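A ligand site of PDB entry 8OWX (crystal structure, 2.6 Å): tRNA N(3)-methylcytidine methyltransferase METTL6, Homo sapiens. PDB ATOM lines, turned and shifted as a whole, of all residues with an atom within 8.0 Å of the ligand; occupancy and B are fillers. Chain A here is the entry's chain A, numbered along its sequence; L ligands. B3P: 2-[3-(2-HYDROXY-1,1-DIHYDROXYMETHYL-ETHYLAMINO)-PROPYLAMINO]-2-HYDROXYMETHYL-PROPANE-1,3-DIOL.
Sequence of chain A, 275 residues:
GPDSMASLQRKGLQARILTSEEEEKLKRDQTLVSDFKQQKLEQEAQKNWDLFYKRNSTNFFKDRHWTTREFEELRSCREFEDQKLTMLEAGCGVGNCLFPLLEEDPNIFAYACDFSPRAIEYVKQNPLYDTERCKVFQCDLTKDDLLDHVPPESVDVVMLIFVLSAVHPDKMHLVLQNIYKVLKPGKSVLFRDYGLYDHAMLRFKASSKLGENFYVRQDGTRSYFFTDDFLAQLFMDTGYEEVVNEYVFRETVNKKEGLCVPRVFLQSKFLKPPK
The side-chain carboxylate (OD2) of Asp 140 is in hydrogen-bond range of an oxygen (O1) of the ligand.
OD2 of Asp 144 lies within salt-bridge range of N2 of the ligand.
The side-chain amide oxygen (OE1) of Gln 46 sits close to an oxygen (O1) of the ligand (3.4 Å).
O3 of the ligand lies within hydrogen-bond range of NE2 of Gln 138 (3.2 Å).
O of Phe 115 sits at hydrogen-bond distance from NE2 of Gln 46.
The side-chain sulfur of Cys 139 sits close to the backbone carbonyl oxygen of Asp 144 (3.6 Å).
OD2 of Asp 144 sits at hydrogen-bond distance from N of Asp 140 (3.2 Å).
The side-chain hydroxyl (OG1) of Thr 142 is in hydrogen-bond range of the side-chain carboxylate (OD1) of Asp 140 (2.5 Å).
The backbone NH of Lys 143 sits at hydrogen-bond distance from the side-chain carboxylate of Asp 140 (3.2 Å).
Merely in contact with the ligand: Lys 143 (3.3 Å), Asp 148 (3.9 Å) and His 149 (3.9 Å).
Within 4 Å of the ligand: Gln 46, Gln 138, Asp 140, Lys 143, Asp 144, Asp 148 and His 149.
The nearest printed residue that does not touch the ligand is Cys 139 (5.3 Å).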
ATOM      1  N   GLN A  43       6.376  -5.866 -22.451  1.00  0.00           N
ATOM      2  CA  GLN A  43       5.379  -4.784 -22.273  1.00  0.00           C
ATOM      3  C   GLN A  43       4.081  -5.204 -22.961  1.00  0.00           C
ATOM      4  O   GLN A  43       2.998  -4.861 -22.457  1.00  0.00           O
ATOM      5  CB  GLN A  43       5.968  -3.508 -22.871  1.00  0.00           C
ATOM      6  CG  GLN A  43       5.445  -2.232 -22.215  1.00  0.00           C
ATOM      7  CD  GLN A  43       4.127  -1.772 -22.779  1.00  0.00           C
ATOM      8  OE1 GLN A  43       4.041  -1.262 -23.891  1.00  0.00           O
ATOM      9  NE2 GLN A  43       3.095  -1.868 -21.958  1.00  0.00           N
ATOM     10  N   GLN A  46       0.605  -9.276 -22.749  1.00  0.00           N
ATOM     11  CA  GLN A  46      -0.858  -9.476 -22.833  1.00  0.00           C
ATOM     12  C   GLN A  46      -1.391  -9.288 -24.240  1.00  0.00           C
ATOM     13  O   GLN A  46      -2.257 -10.036 -24.691  1.00  0.00           O
ATOM     14  CB  GLN A  46      -1.576  -8.543 -21.878  1.00  0.00           C
ATOM     15  CG  GLN A  46      -3.056  -8.615 -22.117  1.00  0.00           C
ATOM     16  CD  GLN A  46      -3.835  -8.004 -20.991  1.00  0.00           C
ATOM     17  OE1 GLN A  46      -3.262  -7.606 -19.976  1.00  0.00           O
ATOM     18  NE2 GLN A  46      -5.148  -7.982 -21.142  1.00  0.00           N
ATOM     19  N   ASP A 114      -7.530 -15.439 -16.777  1.00  0.00           N
ATOM     20  CA  ASP A 114      -6.521 -15.303 -17.838  1.00  0.00           C
ATOM     21  C   ASP A 114      -6.401 -13.809 -18.115  1.00  0.00           C
ATOM     22  O   ASP A 114      -7.415 -13.113 -18.004  1.00  0.00           O
ATOM     23  CB  ASP A 114      -6.913 -16.021 -19.122  1.00  0.00           C
ATOM     24  CG  ASP A 114      -5.761 -16.141 -20.102  1.00  0.00           C
ATOM     25  OD1 ASP A 114      -5.212 -15.087 -20.514  1.00  0.00           O
ATOM     26  OD2 ASP A 114      -5.400 -17.291 -20.453  1.00  0.00           O
ATOM     27  N   PHE A 115      -5.250 -13.357 -18.530  1.00  0.00           N
ATOM     28  CA  PHE A 115      -5.170 -11.922 -18.797  1.00  0.00           C
ATOM     29  C   PHE A 115      -5.593 -11.535 -20.214  1.00  0.00           C
ATOM     30  O   PHE A 115      -5.626 -10.343 -20.498  1.00  0.00           O
ATOM     31  CB  PHE A 115      -3.787 -11.358 -18.520  1.00  0.00           C
ATOM     32  CG  PHE A 115      -2.720 -11.801 -19.455  1.00  0.00           C
ATOM     33  CD1 PHE A 115      -2.932 -12.792 -20.395  1.00  0.00           C
ATOM     34  CD2 PHE A 115      -1.485 -11.194 -19.382  1.00  0.00           C
ATOM     35  CE1 PHE A 115      -1.922 -13.185 -21.228  1.00  0.00           C
ATOM     36  CE2 PHE A 115      -0.461 -11.589 -20.217  1.00  0.00           C
ATOM     37  CZ  PHE A 115      -0.680 -12.588 -21.137  1.00  0.00           C
ATOM     38  N   SER A 116      -5.891 -12.483 -21.088  1.00  0.00           N
ATOM     39  CA  SER A 116      -6.392 -12.069 -22.414  1.00  0.00           C
ATOM     40  C   SER A 116      -7.892 -11.809 -22.334  1.00  0.00           C
ATOM     41  O   SER A 116      -8.657 -12.715 -21.973  1.00  0.00           O
ATOM     42  CB  SER A 116      -6.142 -13.126 -23.446  1.00  0.00           C
ATOM     43  OG  SER A 116      -7.174 -13.030 -24.413  1.00  0.00           O
ATOM     44  N   PRO A 117      -8.356 -10.583 -22.639  1.00  0.00           N
ATOM     45  CA  PRO A 117      -9.782 -10.361 -22.606  1.00  0.00           C
ATOM     46  C   PRO A 117     -10.551 -11.226 -23.609  1.00  0.00           C
ATOM     47  O   PRO A 117     -11.561 -11.820 -23.239  1.00  0.00           O
ATOM     48  CB  PRO A 117      -9.929  -8.884 -22.956  1.00  0.00           C
ATOM     49  CG  PRO A 117      -8.554  -8.288 -22.844  1.00  0.00           C
ATOM     50  CD  PRO A 117      -7.551  -9.376 -22.625  1.00  0.00           C
ATOM     51  N   PHE A 137     -12.435 -14.498 -14.988  1.00  0.00           N
ATOM     52  CA  PHE A 137     -12.097 -13.067 -14.868  1.00  0.00           C
ATOM     53  C   PHE A 137     -10.705 -12.746 -15.423  1.00  0.00           C
ATOM     54  O   PHE A 137      -9.733 -13.403 -15.054  1.00  0.00           O
ATOM     55  CB  PHE A 137     -12.127 -12.675 -13.395  1.00  0.00           C
ATOM     56  CG  PHE A 137     -11.235 -13.468 -12.480  1.00  0.00           C
ATOM     57  CD1 PHE A 137     -11.643 -14.692 -11.960  1.00  0.00           C
ATOM     58  CD2 PHE A 137      -9.983 -12.989 -12.127  1.00  0.00           C
ATOM     59  CE1 PHE A 137     -10.830 -15.406 -11.100  1.00  0.00           C
ATOM     60  CE2 PHE A 137      -9.161 -13.699 -11.262  1.00  0.00           C
ATOM     61  CZ  PHE A 137      -9.582 -14.915 -10.748  1.00  0.00           C
ATOM     62  N   GLN A 138     -10.614 -11.620 -16.112  1.00  0.00           N
ATOM     63  CA  GLN A 138      -9.303 -11.155 -16.602  1.00  0.00           C
ATOM     64  C   GLN A 138      -8.385 -10.876 -15.432  1.00  0.00           C
ATOM     65  O   GLN A 138      -8.782 -10.126 -14.538  1.00  0.00           O
ATOM     66  CB  GLN A 138      -9.458  -9.889 -17.449  1.00  0.00           C
ATOM     67  CG  GLN A 138      -8.225  -9.436 -18.191  1.00  0.00           C
ATOM     68  CD  GLN A 138      -7.382  -8.449 -17.428  1.00  0.00           C
ATOM     69  OE1 GLN A 138      -6.194  -8.640 -17.209  1.00  0.00           O
ATOM     70  NE2 GLN A 138      -7.986  -7.335 -17.056  1.00  0.00           N
ATOM     71  N   CYS A 139      -7.225 -11.495 -15.420  1.00  0.00           N
ATOM     72  CA  CYS A 139      -6.216 -11.163 -14.415  1.00  0.00           C
ATOM     73  C   CYS A 139      -4.850 -11.378 -15.057  1.00  0.00           C
ATOM     74  O   CYS A 139      -4.601 -12.467 -15.578  1.00  0.00           O
ATOM     75  CB  CYS A 139      -6.353 -12.028 -13.159  1.00  0.00           C
ATOM     76  SG  CYS A 139      -4.908 -11.902 -12.063  1.00  0.00           S
ATOM     77  N   ASP A 140      -4.012 -10.379 -14.977  1.00  0.00           N
ATOM     78  CA  ASP A 140      -2.603 -10.586 -15.289  1.00  0.00           C
ATOM     79  C   ASP A 140      -2.028 -11.006 -13.938  1.00  0.00           C
ATOM     80  O   ASP A 140      -1.908 -10.175 -13.033  1.00  0.00           O
ATOM     81  CB  ASP A 140      -1.964  -9.320 -15.811  1.00  0.00           C
ATOM     82  CG  ASP A 140      -0.463  -9.414 -15.968  1.00  0.00           C
ATOM     83  OD1 ASP A 140       0.200 -10.064 -15.124  1.00  0.00           O
ATOM     84  OD2 ASP A 140       0.069  -8.731 -16.864  1.00  0.00           O
ATOM     85  N   LEU A 141      -1.609 -12.251 -13.848  1.00  0.00           N
ATOM     86  CA  LEU A 141      -1.126 -12.838 -12.578  1.00  0.00           C
ATOM     87  C   LEU A 141       0.153 -12.165 -12.079  1.00  0.00           C
ATOM     88  O   LEU A 141       0.500 -12.360 -10.926  1.00  0.00           O
ATOM     89  CB  LEU A 141      -0.959 -14.341 -12.724  1.00  0.00           C
ATOM     90  CG  LEU A 141      -2.200 -15.218 -12.613  1.00  0.00           C
ATOM     91  CD1 LEU A 141      -3.357 -14.547 -13.257  1.00  0.00           C
ATOM     92  CD2 LEU A 141      -1.977 -16.511 -13.374  1.00  0.00           C
ATOM     93  N   THR A 142       0.836 -11.388 -12.903  1.00  0.00           N
ATOM     94  CA  THR A 142       2.040 -10.761 -12.354  1.00  0.00           C
ATOM     95  C   THR A 142       1.666  -9.375 -11.888  1.00  0.00           C
ATOM     96  O   THR A 142       2.500  -8.706 -11.347  1.00  0.00           O
ATOM     97  CB  THR A 142       3.117 -10.539 -13.411  1.00  0.00           C
ATOM     98  OG1 THR A 142       2.564  -9.705 -14.405  1.00  0.00           O
ATOM     99  CG2 THR A 142       3.560 -11.808 -14.080  1.00  0.00           C
ATOM    100  N   LYS A 143       0.431  -9.001 -12.071  1.00  0.00           N
ATOM    101  CA  LYS A 143       0.050  -7.621 -11.710  1.00  0.00           C
ATOM    102  C   LYS A 143      -1.153  -7.535 -10.793  1.00  0.00           C
ATOM    103  O   LYS A 143      -1.149  -6.696  -9.901  1.00  0.00           O
ATOM    104  CB  LYS A 143      -0.244  -6.862 -13.010  1.00  0.00           C
ATOM    105  CG  LYS A 143       0.916  -6.682 -13.979  1.00  0.00           C
ATOM    106  CD  LYS A 143       0.486  -5.970 -15.249  1.00  0.00           C
ATOM    107  CE  LYS A 143       1.649  -5.794 -16.193  1.00  0.00           C
ATOM    108  NZ  LYS A 143       2.780  -5.083 -15.541  1.00  0.00           N
ATOM    109  N   ASP A 144      -2.124  -8.417 -10.949  1.00  0.00           N
ATOM    110  CA  ASP A 144      -3.392  -8.284 -10.213  1.00  0.00           C
ATOM    111  C   ASP A 144      -3.422  -9.249  -9.046  1.00  0.00           C
ATOM    112  O   ASP A 144      -3.202 -10.447  -9.229  1.00  0.00           O
ATOM    113  CB  ASP A 144      -4.534  -8.591 -11.159  1.00  0.00           C
ATOM    114  CG  ASP A 144      -4.534  -7.688 -12.360  1.00  0.00           C
ATOM    115  OD1 ASP A 144      -3.700  -6.763 -12.379  1.00  0.00           O
ATOM    116  OD2 ASP A 144      -5.314  -7.971 -13.290  1.00  0.00           O
ATOM    117  N   ASP A 145      -3.694  -8.716  -7.867  1.00  0.00           N
ATOM    118  CA  ASP A 145      -3.831  -9.572  -6.671  1.00  0.00           C
ATOM    119  C   ASP A 145      -5.046 -10.471  -6.899  1.00  0.00           C
ATOM    120  O   ASP A 145      -6.113  -9.995  -7.280  1.00  0.00           O
ATOM    121  CB  ASP A 145      -3.964  -8.705  -5.413  1.00  0.00           C
ATOM    122  CG  ASP A 145      -4.058  -9.512  -4.125  1.00  0.00           C
ATOM    123  OD1 ASP A 145      -4.953 -10.358  -4.074  1.00  0.00           O
ATOM    124  OD2 ASP A 145      -3.269  -9.276  -3.170  1.00  0.00           O
ATOM    125  N   ASP A 148      -8.614 -10.126  -5.343  1.00  0.00           N
ATOM    126  CA  ASP A 148      -9.711  -9.328  -5.930  1.00  0.00           C
ATOM    127  C   ASP A 148     -10.891 -10.234  -6.274  1.00  0.00           C
ATOM    128  O   ASP A 148     -12.018  -9.740  -6.293  1.00  0.00           O
ATOM    129  CB  ASP A 148      -9.261  -8.611  -7.187  1.00  0.00           C
ATOM    130  CG  ASP A 148      -8.270  -7.511  -6.917  1.00  0.00           C
ATOM    131  OD1 ASP A 148      -7.982  -7.283  -5.721  1.00  0.00           O
ATOM    132  OD2 ASP A 148      -7.766  -6.925  -7.893  1.00  0.00           O
ATOM    133  N   HIS A 149     -10.630 -11.463  -6.719  1.00  0.00           N
ATOM    134  CA  HIS A 149     -11.747 -12.323  -7.141  1.00  0.00           C
ATOM    135  C   HIS A 149     -11.857 -13.655  -6.401  1.00  0.00           C
ATOM    136  O   HIS A 149     -12.919 -14.267  -6.482  1.00  0.00           O
ATOM    137  CB  HIS A 149     -11.646 -12.644  -8.625  1.00  0.00           C
ATOM    138  CG  HIS A 149     -11.468 -11.465  -9.522  1.00  0.00           C
ATOM    139  ND1 HIS A 149     -10.291 -10.752  -9.600  1.00  0.00           N
ATOM    140  CD2 HIS A 149     -12.273 -10.955 -10.467  1.00  0.00           C
ATOM    141  CE1 HIS A 149     -10.415  -9.810 -10.521  1.00  0.00           C
ATOM    142  NE2 HIS A 149     -11.609  -9.906 -11.044  1.00  0.00           N
HETATM  143  C1  B3P L   1      -7.227  -5.909 -14.096  1.00  0.00           C
HETATM  144  C2  B3P L   1      -5.871  -5.336 -14.452  1.00  0.00           C
HETATM  145  C3  B3P L   1      -7.853  -5.072 -13.021  1.00  0.00           C
HETATM  146  N1  B3P L   1      -9.185  -5.554 -12.673  1.00  0.00           N
HETATM  147  C4  B3P L   1      -9.843  -4.652 -11.717  1.00  0.00           C
HETATM  148  C5  B3P L   1     -10.325  -5.462 -10.510  1.00  0.00           C
HETATM  149  C6  B3P L   1     -11.056  -3.990 -12.386  1.00  0.00           C
HETATM  150  C7  B3P L   1      -8.906  -3.548 -11.238  1.00  0.00           C
HETATM  151  N2  B3P L   1      -5.204  -6.067 -15.534  1.00  0.00           N
HETATM  152  C8  B3P L   1      -4.267  -5.261 -16.344  1.00  0.00           C
HETATM  153  C9  B3P L   1      -3.495  -6.168 -17.312  1.00  0.00           C
HETATM  154  C10 B3P L   1      -3.316  -4.420 -15.478  1.00  0.00           C
HETATM  155  C11 B3P L   1      -5.066  -4.234 -17.166  1.00  0.00           C
HETATM  156  O1  B3P L   1      -2.089  -6.016 -17.264  1.00  0.00           O
HETATM  157  O2  B3P L   1      -3.032  -4.982 -14.210  1.00  0.00           O
HETATM  158  O3  B3P L   1      -6.434  -4.561 -17.337  1.00  0.00           O
HETATM  159  O4  B3P L   1     -11.617  -5.982 -10.767  1.00  0.00           O
HETATM  160  O5  B3P L   1     -12.092  -4.927 -12.683  1.00  0.00           O
HETATM  161  O6  B3P L   1      -8.952  -3.466  -9.827  1.00  0.00           O
